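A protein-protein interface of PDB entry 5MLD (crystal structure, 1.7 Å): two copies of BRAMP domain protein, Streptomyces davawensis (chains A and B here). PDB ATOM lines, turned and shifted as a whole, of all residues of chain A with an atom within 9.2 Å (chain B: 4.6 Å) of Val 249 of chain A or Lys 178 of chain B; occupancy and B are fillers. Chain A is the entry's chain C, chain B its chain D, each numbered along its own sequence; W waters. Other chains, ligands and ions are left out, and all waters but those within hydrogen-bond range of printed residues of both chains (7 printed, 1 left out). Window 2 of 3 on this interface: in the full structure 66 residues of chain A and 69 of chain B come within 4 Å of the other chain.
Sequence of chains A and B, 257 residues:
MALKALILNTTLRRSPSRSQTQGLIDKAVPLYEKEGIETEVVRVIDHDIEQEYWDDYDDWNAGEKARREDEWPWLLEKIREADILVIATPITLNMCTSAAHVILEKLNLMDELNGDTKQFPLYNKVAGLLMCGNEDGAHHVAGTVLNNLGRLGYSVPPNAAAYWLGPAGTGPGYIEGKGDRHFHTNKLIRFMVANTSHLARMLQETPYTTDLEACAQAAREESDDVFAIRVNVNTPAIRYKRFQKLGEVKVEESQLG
Asp 180 of chain B touches Glu 222 of chain A. Glu 222 of chain A touches Arg 181 of chain B. Ser 223 of chain A touches His 182 of chain B. Phe 227 of chain A touches His 182 of chain B. CA of Gly 177 of chain B touches CG2 of Ile 229 of chain A, 3.9 Å away. O of Arg 242 of chain A touches OE1 of Glu 176 of chain B, at 3.9 Å. Val 249 of chain A touches Lys 178 of chain B (O to NZ, 3.6 Å).
No position is printed for both chains.
Of the 18 printed residues of chain A, 7 touch a printed residue of chain B. Hydrophobic or aromatic side chains of chain A that line the printed part of chain B: Phe 227 and Ile 229. Of the 9 printed residues of chain B, 6 touch a printed residue of chain A. Among the printed residues, Asp or Glu carboxylates within 4 Å of a Lys or Arg side-chain nitrogen of the other chain: Asp 224 of chain A with Arg 181 of chain B (2.8 Å).
Of the printed residues of chain B, Arg 242 of chain A touches Glu 176. Of chain A, only Ile 229 comes within 4 Å of Gly 177 of chain B. Of chain A, only Val 249 (3.6 Å) comes within 4 Å of Lys 178 of chain B. No residue of chain A comes within 4 Å of Gly 179 of chain B. Of the printed residues of chain A, Asp 180 of chain B touches Glu 222. The nearest residue of chain A that does not touch Lys 178 of chain B is Lys 250 of chain A (4.4 Å). The nearest printed residue of chain A that does not touch His 182 of chain B is Asp 224 of chain A (5.1 Å).
Water W2 lies within hydrogen-bond range of the backbone carbonyl oxygen of Arg 242 of chain A (2.8 Å), the backbone NH of Glu 176 of chain B (2.8 Å) and the backbone NH of Ile 175 of chain B (3.4 Å). Water W6 lies within hydrogen-bond range of the side-chain carboxylate (OE1) of Glu 176 of chain B and the backbone NH (N) of Leu 246 of chain A. Water W7 bridges O of Glu 222 of chain A and O of Asp 180 of chain B. Water W4 bridges ND1 of His 182 of chain B (2.9 Å) and O of Val 226 of chain A (3.4 Å). Water W5 lies within hydrogen-bond range of the backbone carbonyl oxygen (O) of Val 249 of chain A, the side-chain amino group (NZ) of Lys 178 of chain B and the backbone carbonyl oxygen (O) of Ala 228 of chain A. Water W3 bridges N of Ala 228 of chain A (3.1 Å) and O of Gly 177 of chain B (3.4 Å).
O of Ser 223 of chain A sits at hydrogen-bond distance from NH2 of Arg 181 of chain B (3.5 Å). NE of Arg 181 of chain B lies within salt-bridge range of OD1 of Asp 224 of chain A (2.8 Å).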
ATOM      1  N   GLU A 222     -12.873  18.298 -35.899  1.00  0.00           N
ATOM      2  CA  GLU A 222     -13.135  18.255 -34.468  1.00  0.00           C
ATOM      3  C   GLU A 222     -11.863  18.165 -33.634  1.00  0.00           C
ATOM      4  O   GLU A 222     -11.943  17.915 -32.427  1.00  0.00           O
ATOM      5  CB  GLU A 222     -14.052  17.075 -34.145  1.00  0.00           C
ATOM      6  CG  GLU A 222     -13.449  15.727 -34.542  1.00  0.00           C
ATOM      7  CD  GLU A 222     -14.434  14.579 -34.427  1.00  0.00           C
ATOM      8  OE1 GLU A 222     -15.508  14.780 -33.830  1.00  0.00           O
ATOM      9  OE2 GLU A 222     -14.133  13.474 -34.935  1.00  0.00           O
ATOM     10  N   SER A 223     -10.695  18.379 -34.239  1.00  0.00           N
ATOM     11  CA  SER A 223      -9.438  18.088 -33.569  1.00  0.00           C
ATOM     12  C   SER A 223      -8.438  19.217 -33.765  1.00  0.00           C
ATOM     13  O   SER A 223      -8.556  20.033 -34.682  1.00  0.00           O
ATOM     14  CB  SER A 223      -8.834  16.774 -34.079  1.00  0.00           C
ATOM     15  OG  SER A 223      -9.806  15.745 -34.058  1.00  0.00           O
ATOM     16  N   ASP A 224      -7.446  19.243 -32.874  1.00  0.00           N
ATOM     17  CA  ASP A 224      -6.301  20.142 -32.969  1.00  0.00           C
ATOM     18  C   ASP A 224      -5.230  19.542 -33.872  1.00  0.00           C
ATOM     19  O   ASP A 224      -5.243  18.344 -34.174  1.00  0.00           O
ATOM     20  CB  ASP A 224      -5.700  20.405 -31.587  1.00  0.00           C
ATOM     21  CG  ASP A 224      -6.717  20.943 -30.596  1.00  0.00           C
ATOM     22  OD1 ASP A 224      -7.629  21.687 -31.016  1.00  0.00           O
ATOM     23  OD2 ASP A 224      -6.604  20.614 -29.395  1.00  0.00           O
ATOM     24  N   ASP A 225      -4.287  20.390 -34.304  1.00  0.00           N
ATOM     25  CA  ASP A 225      -3.125  19.923 -35.054  1.00  0.00           C
ATOM     26  C   ASP A 225      -1.839  20.032 -34.243  1.00  0.00           C
ATOM     27  O   ASP A 225      -0.744  19.948 -34.802  1.00  0.00           O
ATOM     28  CB  ASP A 225      -2.998  20.659 -36.395  1.00  0.00           C
ATOM     29  CG  ASP A 225      -2.841  22.173 -36.252  1.00  0.00           C
ATOM     30  OD1 ASP A 225      -2.638  22.673 -35.127  1.00  0.00           O
ATOM     31  OD2 ASP A 225      -2.911  22.867 -37.290  1.00  0.00           O
ATOM     32  N   VAL A 226      -1.956  20.221 -32.930  1.00  0.00           N
ATOM     33  CA  VAL A 226      -0.820  20.223 -32.022  1.00  0.00           C
ATOM     34  C   VAL A 226      -1.213  19.408 -30.803  1.00  0.00           C
ATOM     35  O   VAL A 226      -2.313  19.579 -30.265  1.00  0.00           O
ATOM     36  CB  VAL A 226      -0.408  21.644 -31.593  1.00  0.00           C
ATOM     37  CG1 VAL A 226       0.709  21.579 -30.566  1.00  0.00           C
ATOM     38  CG2 VAL A 226       0.039  22.462 -32.790  1.00  0.00           C
ATOM     39  N   PHE A 227      -0.330  18.512 -30.381  1.00  0.00           N
ATOM     40  CA  PHE A 227      -0.451  17.852 -29.092  1.00  0.00           C
ATOM     41  C   PHE A 227       0.531  18.500 -28.125  1.00  0.00           C
ATOM     42  O   PHE A 227       1.727  18.586 -28.418  1.00  0.00           O
ATOM     43  CB  PHE A 227      -0.169  16.350 -29.209  1.00  0.00           C
ATOM     44  CG  PHE A 227      -0.260  15.628 -27.898  1.00  0.00           C
ATOM     45  CD1 PHE A 227       0.831  15.563 -27.046  1.00  0.00           C
ATOM     46  CD2 PHE A 227      -1.442  15.018 -27.516  1.00  0.00           C
ATOM     47  CE1 PHE A 227       0.747  14.919 -25.828  1.00  0.00           C
ATOM     48  CE2 PHE A 227      -1.532  14.363 -26.300  1.00  0.00           C
ATOM     49  CZ  PHE A 227      -0.431  14.314 -25.458  1.00  0.00           C
ATOM     50  N   ALA A 228       0.036  18.929 -26.963  1.00  0.00           N
ATOM     51  CA  ALA A 228       0.895  19.599 -25.997  1.00  0.00           C
ATOM     52  C   ALA A 228       0.400  19.334 -24.581  1.00  0.00           C
ATOM     53  O   ALA A 228      -0.803  19.407 -24.314  1.00  0.00           O
ATOM     54  CB  ALA A 228       0.954  21.109 -26.268  1.00  0.00           C
ATOM     55  N   ILE A 229       1.334  19.018 -23.681  1.00  0.00           N
ATOM     56  CA  ILE A 229       1.022  18.810 -22.270  1.00  0.00           C
ATOM     57  C   ILE A 229       2.207  19.266 -21.442  1.00  0.00           C
ATOM     58  O   ILE A 229       3.358  19.188 -21.881  1.00  0.00           O
ATOM     59  CB  ILE A 229       0.706  17.337 -21.926  1.00  0.00           C
ATOM     60  CG1 ILE A 229       1.802  16.427 -22.482  1.00  0.00           C
ATOM     61  CG2 ILE A 229      -0.698  16.952 -22.366  1.00  0.00           C
ATOM     62  CD1 ILE A 229       1.926  15.148 -21.742  1.00  0.00           C
ATOM     63  N   ARG A 230       1.922  19.708 -20.221  1.00  0.00           N
ATOM     64  CA  ARG A 230       2.977  19.965 -19.258  1.00  0.00           C
ATOM     65  C   ARG A 230       3.373  18.679 -18.544  1.00  0.00           C
ATOM     66  O   ARG A 230       2.599  17.720 -18.436  1.00  0.00           O
ATOM     67  CB  ARG A 230       2.543  21.022 -18.243  1.00  0.00           C
ATOM     68  CG  ARG A 230       2.318  22.364 -18.887  1.00  0.00           C
ATOM     69  CD  ARG A 230       2.146  23.515 -17.910  1.00  0.00           C
ATOM     70  NE  ARG A 230       1.856  24.737 -18.657  1.00  0.00           N
ATOM     71  CZ  ARG A 230       2.780  25.484 -19.258  1.00  0.00           C
ATOM     72  NH1 ARG A 230       4.061  25.143 -19.190  1.00  0.00           N
ATOM     73  NH2 ARG A 230       2.424  26.572 -19.930  1.00  0.00           N
ATOM     74  N   VAL A 231       4.594  18.679 -18.039  1.00  0.00           N
ATOM     75  CA  VAL A 231       5.201  17.509 -17.428  1.00  0.00           C
ATOM     76  C   VAL A 231       5.625  17.878 -16.018  1.00  0.00           C
ATOM     77  O   VAL A 231       6.195  18.951 -15.796  1.00  0.00           O
ATOM     78  CB  VAL A 231       6.407  17.024 -18.264  1.00  0.00           C
ATOM     79  CG1 VAL A 231       7.058  15.804 -17.623  1.00  0.00           C
ATOM     80  CG2 VAL A 231       5.970  16.757 -19.705  1.00  0.00           C
ATOM     81  N   ARG A 242      -3.804  10.469 -13.582  1.00  0.00           N
ATOM     82  CA  ARG A 242      -4.591  10.910 -14.725  1.00  0.00           C
ATOM     83  C   ARG A 242      -4.917  12.398 -14.658  1.00  0.00           C
ATOM     84  O   ARG A 242      -5.201  12.996 -15.697  1.00  0.00           O
ATOM     85  CB  ARG A 242      -5.873  10.085 -14.812  1.00  0.00           C
ATOM     86  CG  ARG A 242      -6.908  10.470 -13.761  1.00  0.00           C
ATOM     87  CD  ARG A 242      -7.749   9.287 -13.316  1.00  0.00           C
ATOM     88  NE  ARG A 242      -8.687   9.682 -12.270  1.00  0.00           N
ATOM     89  CZ  ARG A 242      -8.370   9.810 -10.982  1.00  0.00           C
ATOM     90  NH1 ARG A 242      -7.134   9.571 -10.562  1.00  0.00           N
ATOM     91  NH2 ARG A 242      -9.295  10.179 -10.105  1.00  0.00           N
ATOM     92  N   LEU A 246      -1.099  20.760 -13.552  1.00  0.00           N
ATOM     93  CA  LEU A 246       0.103  21.421 -14.029  1.00  0.00           C
ATOM     94  C   LEU A 246      -0.184  22.660 -14.855  1.00  0.00           C
ATOM     95  O   LEU A 246       0.710  23.498 -15.023  1.00  0.00           O
ATOM     96  CB  LEU A 246       0.941  20.453 -14.870  1.00  0.00           C
ATOM     97  CG  LEU A 246       1.376  19.178 -14.149  1.00  0.00           C
ATOM     98  CD1 LEU A 246       1.985  18.213 -15.145  1.00  0.00           C
ATOM     99  CD2 LEU A 246       2.350  19.491 -13.027  1.00  0.00           C
ATOM    100  N   GLY A 247      -1.392  22.800 -15.358  1.00  0.00           N
ATOM    101  CA  GLY A 247      -1.717  23.921 -16.208  1.00  0.00           C
ATOM    102  C   GLY A 247      -1.783  23.513 -17.665  1.00  0.00           C
ATOM    103  O   GLY A 247      -1.086  22.600 -18.121  1.00  0.00           O
ATOM    104  N   GLU A 248      -2.656  24.180 -18.405  1.00  0.00           N
ATOM    105  CA  GLU A 248      -2.738  23.969 -19.838  1.00  0.00           C
ATOM    106  C   GLU A 248      -1.551  24.622 -20.535  1.00  0.00           C
ATOM    107  O   GLU A 248      -0.987  25.611 -20.056  1.00  0.00           O
ATOM    108  CB  GLU A 248      -4.044  24.550 -20.376  1.00  0.00           C
ATOM    109  CG  GLU A 248      -4.330  25.938 -19.809  1.00  0.00           C
ATOM    110  CD  GLU A 248      -5.547  26.599 -20.423  1.00  0.00           C
ATOM    111  OE1 GLU A 248      -6.682  26.187 -20.095  1.00  0.00           O
ATOM    112  OE2 GLU A 248      -5.369  27.539 -21.227  1.00  0.00           O
ATOM    113  N   VAL A 249      -1.162  24.049 -21.671  1.00  0.00           N
ATOM    114  CA  VAL A 249      -0.182  24.654 -22.564  1.00  0.00           C
ATOM    115  C   VAL A 249      -0.944  25.344 -23.680  1.00  0.00           C
ATOM    116  O   VAL A 249      -1.827  24.741 -24.303  1.00  0.00           O
ATOM    117  CB  VAL A 249       0.785  23.610 -23.148  1.00  0.00           C
ATOM    118  CG1 VAL A 249       2.017  24.294 -23.735  1.00  0.00           C
ATOM    119  CG2 VAL A 249       1.171  22.601 -22.108  1.00  0.00           C
ATOM    120  N   LYS A 250      -0.613  26.601 -23.935  1.00  0.00           N
ATOM    121  CA  LYS A 250      -1.215  27.342 -25.031  1.00  0.00           C
ATOM    122  C   LYS A 250      -0.188  27.495 -26.141  1.00  0.00           C
ATOM    123  O   LYS A 250       0.939  27.942 -25.899  1.00  0.00           O
ATOM    124  CB  LYS A 250      -1.736  28.700 -24.553  1.00  0.00           C
ATOM    125  CG  LYS A 250      -2.898  29.245 -25.375  1.00  0.00           C
ATOM    126  CD  LYS A 250      -3.997  28.203 -25.614  1.00  0.00           C
ATOM    127  CE  LYS A 250      -4.547  27.594 -24.319  1.00  0.00           C
ATOM    128  NZ  LYS A 250      -4.817  28.610 -23.268  1.00  0.00           N
ATOM    129  N   VAL A 251      -0.570  27.091 -27.343  1.00  0.00           N
ATOM    130  CA  VAL A 251       0.298  27.147 -28.508  1.00  0.00           C
ATOM    131  C   VAL A 251       0.006  28.434 -29.264  1.00  0.00           C
ATOM    132  O   VAL A 251      -1.093  28.996 -29.178  1.00  0.00           O
ATOM    133  CB  VAL A 251       0.108  25.901 -29.400  1.00  0.00           C
ATOM    134  CG1 VAL A 251       0.103  24.648 -28.534  1.00  0.00           C
ATOM    135  CG2 VAL A 251      -1.179  26.005 -30.211  1.00  0.00           C
ATOM    136  N   GLU A 252       1.000  28.913 -30.008  1.00  0.00           N
ATOM    137  CA  GLU A 252       0.924  30.237 -30.612  1.00  0.00           C
ATOM    138  C   GLU A 252       0.357  30.243 -32.026  1.00  0.00           C
ATOM    139  O   GLU A 252       0.250  31.319 -32.625  1.00  0.00           O
ATOM    140  CB  GLU A 252       2.303  30.896 -30.608  1.00  0.00           C
ATOM    141  CG  GLU A 252       2.555  31.718 -29.361  1.00  0.00           C
ATOM    142  CD  GLU A 252       3.748  32.631 -29.503  1.00  0.00           C
ATOM    143  OE1 GLU A 252       4.180  32.867 -30.653  1.00  0.00           O
ATOM    144  OE2 GLU A 252       4.257  33.107 -28.467  1.00  0.00           O
ATOM    145  N   TYR B 174      -6.831  11.469 -20.620  1.00  0.00           N
ATOM    146  CA  TYR B 174      -7.591  11.970 -21.759  1.00  0.00           C
ATOM    147  C   TYR B 174      -8.137  13.375 -21.523  1.00  0.00           C
ATOM    148  O   TYR B 174      -8.096  14.223 -22.425  1.00  0.00           O
ATOM    149  CB  TYR B 174      -8.723  10.991 -22.033  1.00  0.00           C
ATOM    150  CG  TYR B 174      -9.632  11.273 -23.205  1.00  0.00           C
ATOM    151  CD1 TYR B 174      -9.327  10.799 -24.482  1.00  0.00           C
ATOM    152  CD2 TYR B 174     -10.833  11.942 -23.025  1.00  0.00           C
ATOM    153  CE1 TYR B 174     -10.190  11.013 -25.547  1.00  0.00           C
ATOM    154  CE2 TYR B 174     -11.696  12.155 -24.077  1.00  0.00           C
ATOM    155  CZ  TYR B 174     -11.370  11.699 -25.333  1.00  0.00           C
ATOM    156  OH  TYR B 174     -12.245  11.926 -26.378  1.00  0.00           O
ATOM    157  N   ILE B 175      -8.675  13.639 -20.332  1.00  0.00           N
ATOM    158  CA  ILE B 175      -9.378  14.904 -20.112  1.00  0.00           C
ATOM    159  C   ILE B 175      -8.388  16.069 -20.075  1.00  0.00           C
ATOM    160  O   ILE B 175      -8.472  17.002 -20.886  1.00  0.00           O
ATOM    161  CB  ILE B 175     -10.244  14.826 -18.841  1.00  0.00           C
ATOM    162  CG1 ILE B 175     -11.408  13.857 -19.082  1.00  0.00           C
ATOM    163  CG2 ILE B 175     -10.761  16.210 -18.463  1.00  0.00           C
ATOM    164  CD1 ILE B 175     -12.118  13.353 -17.826  1.00  0.00           C
ATOM    165  N   GLU B 176      -7.403  16.006 -19.170  1.00  0.00           N
ATOM    166  CA  GLU B 176      -6.407  17.080 -19.082  1.00  0.00           C
ATOM    167  C   GLU B 176      -5.503  17.134 -20.310  1.00  0.00           C
ATOM    168  O   GLU B 176      -5.000  18.209 -20.657  1.00  0.00           O
ATOM    169  CB  GLU B 176      -5.551  16.930 -17.824  1.00  0.00           C
ATOM    170  CG  GLU B 176      -6.193  17.456 -16.536  1.00  0.00           C
ATOM    171  CD  GLU B 176      -5.256  17.381 -15.338  1.00  0.00           C
ATOM    172  OE1 GLU B 176      -4.162  16.798 -15.471  1.00  0.00           O
ATOM    173  OE2 GLU B 176      -5.603  17.907 -14.259  1.00  0.00           O
ATOM    174  N   GLY B 177      -5.276  16.002 -20.976  1.00  0.00           N
ATOM    175  CA  GLY B 177      -4.490  15.959 -22.194  1.00  0.00           C
ATOM    176  C   GLY B 177      -5.221  16.359 -23.451  1.00  0.00           C
ATOM    177  O   GLY B 177      -4.636  16.305 -24.538  1.00  0.00           O
ATOM    178  N   LYS B 178      -6.488  16.763 -23.322  1.00  0.00           N
ATOM    179  CA  LYS B 178      -7.307  17.273 -24.427  1.00  0.00           C
ATOM    180  C   LYS B 178      -7.529  16.208 -25.494  1.00  0.00           C
ATOM    181  O   LYS B 178      -7.540  16.488 -26.696  1.00  0.00           O
ATOM    182  CB  LYS B 178      -6.705  18.543 -25.031  1.00  0.00           C
ATOM    183  CG  LYS B 178      -6.636  19.707 -24.051  1.00  0.00           C
ATOM    184  CD  LYS B 178      -5.766  20.820 -24.631  1.00  0.00           C
ATOM    185  CE  LYS B 178      -5.839  22.109 -23.831  1.00  0.00           C
ATOM    186  NZ  LYS B 178      -5.065  23.199 -24.506  1.00  0.00           N
ATOM    187  N   GLY B 179      -7.729  14.970 -25.041  1.00  0.00           N
ATOM    188  CA  GLY B 179      -7.936  13.875 -25.959  1.00  0.00           C
ATOM    189  C   GLY B 179      -9.190  13.993 -26.786  1.00  0.00           C
ATOM    190  O   GLY B 179      -9.271  13.378 -27.855  1.00  0.00           O
ATOM    191  N   ASP B 180     -10.182  14.767 -26.326  1.00  0.00           N
ATOM    192  CA  ASP B 180     -11.393  14.891 -27.136  1.00  0.00           C
ATOM    193  C   ASP B 180     -11.125  15.639 -28.431  1.00  0.00           C
ATOM    194  O   ASP B 180     -11.937  15.559 -29.358  1.00  0.00           O
ATOM    195  CB  ASP B 180     -12.524  15.574 -26.360  1.00  0.00           C
ATOM    196  CG  ASP B 180     -12.289  17.049 -26.156  1.00  0.00           C
ATOM    197  OD1 ASP B 180     -11.218  17.420 -25.631  1.00  0.00           O
ATOM    198  OD2 ASP B 180     -13.180  17.845 -26.536  1.00  0.00           O
ATOM    199  N   ARG B 181      -9.995  16.337 -28.520  1.00  0.00           N
ATOM    200  CA  ARG B 181      -9.581  16.998 -29.750  1.00  0.00           C
ATOM    201  C   ARG B 181      -8.310  16.378 -30.329  1.00  0.00           C
ATOM    202  O   ARG B 181      -7.576  17.036 -31.075  1.00  0.00           O
ATOM    203  CB  ARG B 181      -9.420  18.501 -29.497  1.00  0.00           C
ATOM    204  CG  ARG B 181     -10.725  19.150 -29.011  1.00  0.00           C
ATOM    205  CD  ARG B 181     -10.673  20.674 -29.038  1.00  0.00           C
ATOM    206  NE  ARG B 181     -10.282  21.169 -30.357  1.00  0.00           N
ATOM    207  CZ  ARG B 181     -11.110  21.390 -31.370  1.00  0.00           C
ATOM    208  NH1 ARG B 181     -12.414  21.181 -31.241  1.00  0.00           N
ATOM    209  NH2 ARG B 181     -10.628  21.837 -32.519  1.00  0.00           N
ATOM    210  N   HIS B 182      -8.050  15.110 -30.024  1.00  0.00           N
ATOM    211  CA  HIS B 182      -6.876  14.407 -30.533  1.00  0.00           C
ATOM    212  C   HIS B 182      -7.229  13.758 -31.865  1.00  0.00           C
ATOM    213  O   HIS B 182      -8.032  12.822 -31.915  1.00  0.00           O
ATOM    214  CB  HIS B 182      -6.408  13.365 -29.524  1.00  0.00           C
ATOM    215  CG  HIS B 182      -5.026  12.848 -29.784  1.00  0.00           C
ATOM    216  ND1 HIS B 182      -3.904  13.646 -29.708  1.00  0.00           N
ATOM    217  CD2 HIS B 182      -4.586  11.605 -30.093  1.00  0.00           C
ATOM    218  CE1 HIS B 182      -2.831  12.918 -29.968  1.00  0.00           C
ATOM    219  NE2 HIS B 182      -3.219  11.677 -30.206  1.00  0.00           N
HETATM  220  O   HOH W   1      -3.033  21.205 -26.079  1.00  0.00           O
HETATM  221  O   HOH W   2      -7.258  13.949 -17.284  1.00  0.00           O
HETATM  222  O   HOH W   3      -3.038  18.531 -26.582  1.00  0.00           O
HETATM  223  O   HOH W   4      -3.708  16.484 -30.100  1.00  0.00           O
HETATM  224  O   HOH W   5      -2.588  22.070 -23.464  1.00  0.00           O
HETATM  225  O   HOH W   6      -2.123  18.694 -15.677  1.00  0.00           O
HETATM  226  O   HOH W   7     -14.052  17.498 -30.631  1.00  0.00           O
